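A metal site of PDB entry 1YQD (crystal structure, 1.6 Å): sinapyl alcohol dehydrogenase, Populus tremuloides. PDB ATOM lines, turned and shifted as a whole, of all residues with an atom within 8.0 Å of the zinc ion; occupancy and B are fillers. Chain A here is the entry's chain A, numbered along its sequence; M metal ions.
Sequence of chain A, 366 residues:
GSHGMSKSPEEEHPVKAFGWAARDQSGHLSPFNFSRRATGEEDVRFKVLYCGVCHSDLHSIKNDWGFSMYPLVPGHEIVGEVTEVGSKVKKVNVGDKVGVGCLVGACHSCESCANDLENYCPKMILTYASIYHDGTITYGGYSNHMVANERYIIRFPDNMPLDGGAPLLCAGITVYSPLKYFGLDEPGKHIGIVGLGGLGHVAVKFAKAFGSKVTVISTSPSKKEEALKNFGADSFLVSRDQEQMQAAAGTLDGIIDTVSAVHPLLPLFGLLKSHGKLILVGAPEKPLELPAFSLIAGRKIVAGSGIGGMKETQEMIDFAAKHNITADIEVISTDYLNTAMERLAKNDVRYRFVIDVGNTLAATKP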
ATOM      1  N   GLY A 105       5.905  -9.823 -24.016  1.00  0.00           N
ATOM      2  CA  GLY A 105       4.657  -9.930 -23.277  1.00  0.00           C
ATOM      3  C   GLY A 105       4.281 -11.320 -22.818  1.00  0.00           C
ATOM      4  O   GLY A 105       4.907 -12.314 -23.187  1.00  0.00           O
ATOM      5  N   ALA A 106       3.238 -11.369 -21.986  1.00  0.00           N
ATOM      6  CA  ALA A 106       2.695 -12.609 -21.423  1.00  0.00           C
ATOM      7  C   ALA A 106       1.362 -12.239 -20.773  1.00  0.00           C
ATOM      8  O   ALA A 106       0.969 -11.071 -20.806  1.00  0.00           O
ATOM      9  CB  ALA A 106       3.653 -13.198 -20.396  1.00  0.00           C
ATOM     10  N   CYS A 107       0.683 -13.210 -20.163  1.00  0.00           N
ATOM     11  CA  CYS A 107      -0.622 -12.941 -19.560  1.00  0.00           C
ATOM     12  C   CYS A 107      -0.607 -12.156 -18.256  1.00  0.00           C
ATOM     13  O   CYS A 107      -1.553 -11.417 -17.967  1.00  0.00           O
ATOM     14  CB  CYS A 107      -1.419 -14.246 -19.388  1.00  0.00           C
ATOM     15  SG  CYS A 107      -1.157 -15.197 -17.860  1.00  0.00           S
ATOM     16  N   HIS A 108       0.454 -12.316 -17.462  1.00  0.00           N
ATOM     17  CA  HIS A 108       0.587 -11.613 -16.191  1.00  0.00           C
ATOM     18  C   HIS A 108      -0.491 -12.009 -15.180  1.00  0.00           C
ATOM     19  O   HIS A 108      -0.731 -11.284 -14.216  1.00  0.00           O
ATOM     20  CB  HIS A 108       0.518 -10.094 -16.407  1.00  0.00           C
ATOM     21  CG  HIS A 108       1.646  -9.538 -17.202  1.00  0.00           C
ATOM     22  ND1 HIS A 108       2.594 -10.330 -17.802  1.00  0.00           N
ATOM     23  CD2 HIS A 108       1.979  -8.257 -17.489  1.00  0.00           C
ATOM     24  CE1 HIS A 108       3.470  -9.564 -18.441  1.00  0.00           C
ATOM     25  NE2 HIS A 108       3.118  -8.302 -18.275  1.00  0.00           N
ATOM     26  N   SER A 109      -1.137 -13.155 -15.394  1.00  0.00           N
ATOM     27  CA  SER A 109      -2.173 -13.591 -14.464  1.00  0.00           C
ATOM     28  C   SER A 109      -2.176 -15.096 -14.210  1.00  0.00           C
ATOM     29  O   SER A 109      -3.202 -15.654 -13.823  1.00  0.00           O
ATOM     30  CB  SER A 109      -3.556 -13.157 -14.976  1.00  0.00           C
ATOM     31  OG  SER A 109      -3.869 -13.769 -16.205  1.00  0.00           O
ATOM     32  N   CYS A 110      -1.045 -15.744 -14.450  1.00  0.00           N
ATOM     33  CA  CYS A 110      -0.949 -17.183 -14.212  1.00  0.00           C
ATOM     34  C   CYS A 110       0.198 -17.449 -13.248  1.00  0.00           C
ATOM     35  O   CYS A 110       1.004 -16.559 -12.957  1.00  0.00           O
ATOM     36  CB  CYS A 110      -0.715 -17.941 -15.517  1.00  0.00           C
ATOM     37  SG  CYS A 110       0.956 -17.818 -16.180  1.00  0.00           S
ATOM     38  N   GLU A 111       0.279 -18.681 -12.747  1.00  0.00           N
ATOM     39  CA  GLU A 111       1.330 -19.048 -11.797  1.00  0.00           C
ATOM     40  C   GLU A 111       2.732 -18.877 -12.390  1.00  0.00           C
ATOM     41  O   GLU A 111       3.660 -18.472 -11.697  1.00  0.00           O
ATOM     42  CB  GLU A 111       1.146 -20.486 -11.321  1.00  0.00           C
ATOM     43  CG  GLU A 111       1.125 -21.525 -12.429  1.00  0.00           C
ATOM     44  CD  GLU A 111       1.092 -22.950 -11.905  1.00  0.00           C
ATOM     45  OE1 GLU A 111       0.979 -23.884 -12.732  1.00  0.00           O
ATOM     46  OE2 GLU A 111       1.166 -23.139 -10.673  1.00  0.00           O
ATOM     47  N   SER A 112       2.880 -19.169 -13.673  1.00  0.00           N
ATOM     48  CA  SER A 112       4.185 -19.039 -14.324  1.00  0.00           C
ATOM     49  C   SER A 112       4.652 -17.588 -14.325  1.00  0.00           C
ATOM     50  O   SER A 112       5.782 -17.284 -13.948  1.00  0.00           O
ATOM     51  CB  SER A 112       4.112 -19.578 -15.756  1.00  0.00           C
ATOM     52  OG  SER A 112       5.418 -19.810 -16.266  1.00  0.00           O
ATOM     53  N   CYS A 113       3.778 -16.674 -14.738  1.00  0.00           N
ATOM     54  CA  CYS A 113       4.127 -15.253 -14.758  1.00  0.00           C
ATOM     55  C   CYS A 113       4.410 -14.749 -13.347  1.00  0.00           C
ATOM     56  O   CYS A 113       5.324 -13.965 -13.134  1.00  0.00           O
ATOM     57  CB  CYS A 113       2.999 -14.427 -15.383  1.00  0.00           C
ATOM     58  SG  CYS A 113       2.836 -14.570 -17.172  1.00  0.00           S
ATOM     59  N   ALA A 114       3.605 -15.211 -12.388  1.00  0.00           N
ATOM     60  CA  ALA A 114       3.762 -14.787 -11.009  1.00  0.00           C
ATOM     61  C   ALA A 114       5.103 -15.233 -10.449  1.00  0.00           C
ATOM     62  O   ALA A 114       5.675 -14.577  -9.571  1.00  0.00           O
ATOM     63  CB  ALA A 114       2.634 -15.358 -10.155  1.00  0.00           C
ATOM     64  N   LEU A 117       8.376 -16.395 -14.595  1.00  0.00           N
ATOM     65  CA  LEU A 117       8.647 -17.286 -15.710  1.00  0.00           C
ATOM     66  C   LEU A 117       7.685 -16.963 -16.847  1.00  0.00           C
ATOM     67  O   LEU A 117       6.889 -17.804 -17.264  1.00  0.00           O
ATOM     68  CB  LEU A 117       8.505 -18.749 -15.278  1.00  0.00           C
ATOM     69  CG  LEU A 117       9.580 -19.218 -14.299  1.00  0.00           C
ATOM     70  CD1 LEU A 117       9.271 -20.633 -13.830  1.00  0.00           C
ATOM     71  CD2 LEU A 117      10.944 -19.170 -14.972  1.00  0.00           C
ATOM     72  N   GLU A 118       7.763 -15.728 -17.340  1.00  0.00           N
ATOM     73  CA  GLU A 118       6.898 -15.288 -18.427  1.00  0.00           C
ATOM     74  C   GLU A 118       7.192 -16.129 -19.658  1.00  0.00           C
ATOM     75  O   GLU A 118       6.339 -16.289 -20.534  1.00  0.00           O
ATOM     76  CB  GLU A 118       7.158 -13.813 -18.747  1.00  0.00           C
ATOM     77  CG  GLU A 118       6.894 -12.828 -17.605  1.00  0.00           C
ATOM     78  CD  GLU A 118       8.096 -12.630 -16.693  1.00  0.00           C
ATOM     79  OE1 GLU A 118       8.044 -11.727 -15.832  1.00  0.00           O
ATOM     80  OE2 GLU A 118       9.091 -13.363 -16.824  1.00  0.00           O
ATOM     81  N   ASN A 119       8.410 -16.669 -19.715  1.00  0.00           N
ATOM     82  CA  ASN A 119       8.844 -17.494 -20.836  1.00  0.00           C
ATOM     83  C   ASN A 119       8.113 -18.830 -20.910  1.00  0.00           C
ATOM     84  O   ASN A 119       8.068 -19.455 -21.976  1.00  0.00           O
ATOM     85  CB  ASN A 119      10.354 -17.715 -20.762  1.00  0.00           C
ATOM     86  CG  ASN A 119      10.800 -18.291 -19.425  1.00  0.00           C
ATOM     87  OD1 ASN A 119      10.290 -17.925 -18.372  1.00  0.00           O
ATOM     88  ND2 ASN A 119      11.798 -19.184 -19.471  1.00  0.00           N
ATOM     89  N   TYR A 120       7.540 -19.271 -19.800  1.00  0.00           N
ATOM     90  CA  TYR A 120       6.804 -20.527 -19.787  1.00  0.00           C
ATOM     91  C   TYR A 120       5.304 -20.305 -19.679  1.00  0.00           C
ATOM     92  O   TYR A 120       4.540 -21.238 -19.449  1.00  0.00           O
ATOM     93  CB  TYR A 120       7.321 -21.432 -18.666  1.00  0.00           C
ATOM     94  CG  TYR A 120       8.760 -21.873 -18.892  1.00  0.00           C
ATOM     95  CD1 TYR A 120       9.746 -21.626 -17.944  1.00  0.00           C
ATOM     96  CD2 TYR A 120       9.135 -22.520 -20.081  1.00  0.00           C
ATOM     97  CE1 TYR A 120      11.076 -21.991 -18.167  1.00  0.00           C
ATOM     98  CE2 TYR A 120      10.457 -22.893 -20.311  1.00  0.00           C
ATOM     99  CZ  TYR A 120      11.426 -22.617 -19.354  1.00  0.00           C
ATOM    100  OH  TYR A 120      12.739 -22.961 -19.595  1.00  0.00           O
ATOM    101  N   CYS A 121       4.893 -19.050 -19.854  1.00  0.00           N
ATOM    102  CA  CYS A 121       3.477 -18.706 -19.826  1.00  0.00           C
ATOM    103  C   CYS A 121       2.846 -19.258 -21.097  1.00  0.00           C
ATOM    104  O   CYS A 121       3.415 -19.124 -22.185  1.00  0.00           O
ATOM    105  CB  CYS A 121       3.306 -17.193 -19.792  1.00  0.00           C
ATOM    106  SG  CYS A 121       1.593 -16.645 -19.981  1.00  0.00           S
ATOM    107  N   PRO A 122       1.673 -19.889 -20.992  1.00  0.00           N
ATOM    108  CA  PRO A 122       1.048 -20.426 -22.205  1.00  0.00           C
ATOM    109  C   PRO A 122       0.686 -19.338 -23.216  1.00  0.00           C
ATOM    110  O   PRO A 122       0.535 -19.619 -24.404  1.00  0.00           O
ATOM    111  CB  PRO A 122      -0.184 -21.167 -21.659  1.00  0.00           C
ATOM    112  CG  PRO A 122      -0.492 -20.438 -20.385  1.00  0.00           C
ATOM    113  CD  PRO A 122       0.872 -20.207 -19.799  1.00  0.00           C
ATOM    114  N   LYS A 123       0.577 -18.104 -22.741  1.00  0.00           N
ATOM    115  CA  LYS A 123       0.227 -16.973 -23.598  1.00  0.00           C
ATOM    116  C   LYS A 123       1.397 -16.016 -23.798  1.00  0.00           C
ATOM    117  O   LYS A 123       1.201 -14.835 -24.074  1.00  0.00           O
ATOM    118  CB  LYS A 123      -0.956 -16.218 -23.013  1.00  0.00           C
ATOM    119  CG  LYS A 123      -2.197 -17.071 -22.778  1.00  0.00           C
ATOM    120  CD  LYS A 123      -3.262 -16.289 -22.044  1.00  0.00           C
ATOM    121  CE  LYS A 123      -4.467 -17.155 -21.707  1.00  0.00           C
ATOM    122  NZ  LYS A 123      -5.491 -16.373 -20.952  1.00  0.00           N
ATOM    123  N   MET A 124       2.623 -16.528 -23.662  1.00  0.00           N
ATOM    124  CA  MET A 124       3.800 -15.689 -23.848  1.00  0.00           C
ATOM    125  C   MET A 124       3.805 -15.110 -25.265  1.00  0.00           C
ATOM    126  O   MET A 124       3.318 -15.756 -26.212  1.00  0.00           O
ATOM    127  CB  MET A 124       5.073 -16.511 -23.592  1.00  0.00           C
ATOM    128  CG  MET A 124       5.218 -17.719 -24.475  1.00  0.00           C
ATOM    129  SD  MET A 124       6.311 -17.411 -25.881  1.00  0.00           S
ATOM    130  CE  MET A 124       7.877 -17.919 -25.170  1.00  0.00           C
ATOM    131  N   ARG A 151       8.162  -4.106 -18.213  1.00  0.00           N
ATOM    132  CA  ARG A 151       8.507  -5.395 -17.627  1.00  0.00           C
ATOM    133  C   ARG A 151       9.463  -6.196 -18.504  1.00  0.00           C
ATOM    134  O   ARG A 151      10.163  -7.094 -18.020  1.00  0.00           O
ATOM    135  CB  ARG A 151       7.239  -6.195 -17.370  1.00  0.00           C
ATOM    136  CG  ARG A 151       7.461  -7.561 -16.743  1.00  0.00           C
ATOM    137  CD  ARG A 151       6.129  -8.124 -16.287  1.00  0.00           C
ATOM    138  NE  ARG A 151       6.244  -9.470 -15.742  1.00  0.00           N
ATOM    139  CZ  ARG A 151       5.301 -10.053 -15.003  1.00  0.00           C
ATOM    140  NH1 ARG A 151       4.187  -9.379 -14.730  1.00  0.00           N
ATOM    141  NH2 ARG A 151       5.464 -11.284 -14.556  1.00  0.00           N
ATOM    142  N   TYR A 152       9.503  -5.867 -19.792  1.00  0.00           N
ATOM    143  CA  TYR A 152      10.351  -6.570 -20.748  1.00  0.00           C
ATOM    144  C   TYR A 152      11.581  -5.799 -21.177  1.00  0.00           C
ATOM    145  O   TYR A 152      12.301  -6.194 -22.102  1.00  0.00           O
ATOM    146  CB  TYR A 152       9.500  -6.996 -21.949  1.00  0.00           C
ATOM    147  CG  TYR A 152       8.413  -7.935 -21.520  1.00  0.00           C
ATOM    148  CD1 TYR A 152       7.208  -7.448 -20.981  1.00  0.00           C
ATOM    149  CD2 TYR A 152       8.628  -9.306 -21.503  1.00  0.00           C
ATOM    150  CE1 TYR A 152       6.269  -8.321 -20.429  1.00  0.00           C
ATOM    151  CE2 TYR A 152       7.694 -10.187 -20.948  1.00  0.00           C
ATOM    152  CZ  TYR A 152       6.527  -9.687 -20.414  1.00  0.00           C
ATOM    153  OH  TYR A 152       5.624 -10.552 -19.844  1.00  0.00           O
HETATM  154 ZN    ZN M   1       1.054 -16.048 -17.761  1.00  0.00          ZN
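Residues that only touch the zinc ion: His 108 (3.8 Å). Five residues have an atom within 4 Å of the zinc ion: Cys 107, His 108, Cys 110, Cys 113 and Cys 121. The nearest printed residue that does not touch the zinc ion is Ser 109 (4.3 Å).
The side-chain sulfur (SG) of Cys 121 sits close to the backbone NH (N) of Lys 123, 3.3 Å away. SG of Cys 107 sits close to N of Ser 109. The side-chain sulfur of Cys 110 lies close to the backbone NH of Ser 112 (3.4 Å). The backbone NH of His 108 lies close to the side-chain sulfur of Cys 113, at 3.3 Å. The guanidinium group of Arg 151 is in hydrogen-bond range of the backbone carbonyl oxygen of Cys 113, at 3.0 Å. A ring nitrogen (ND1) of His 108 sits at hydrogen-bond distance from the backbone carbonyl oxygen of Ala 106.
The zinc ion is bound by the side-chain sulfur (SG) of Cys 121 (2.4 Å), the side-chain sulfur (SG) of Cys 107 (2.4 Å), the side-chain sulfur (SG) of Cys 110 (2.4 Å) and the side-chain sulfur (SG) of Cys 113 (2.4 Å). The zinc ion has four donor atoms within binding distance.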
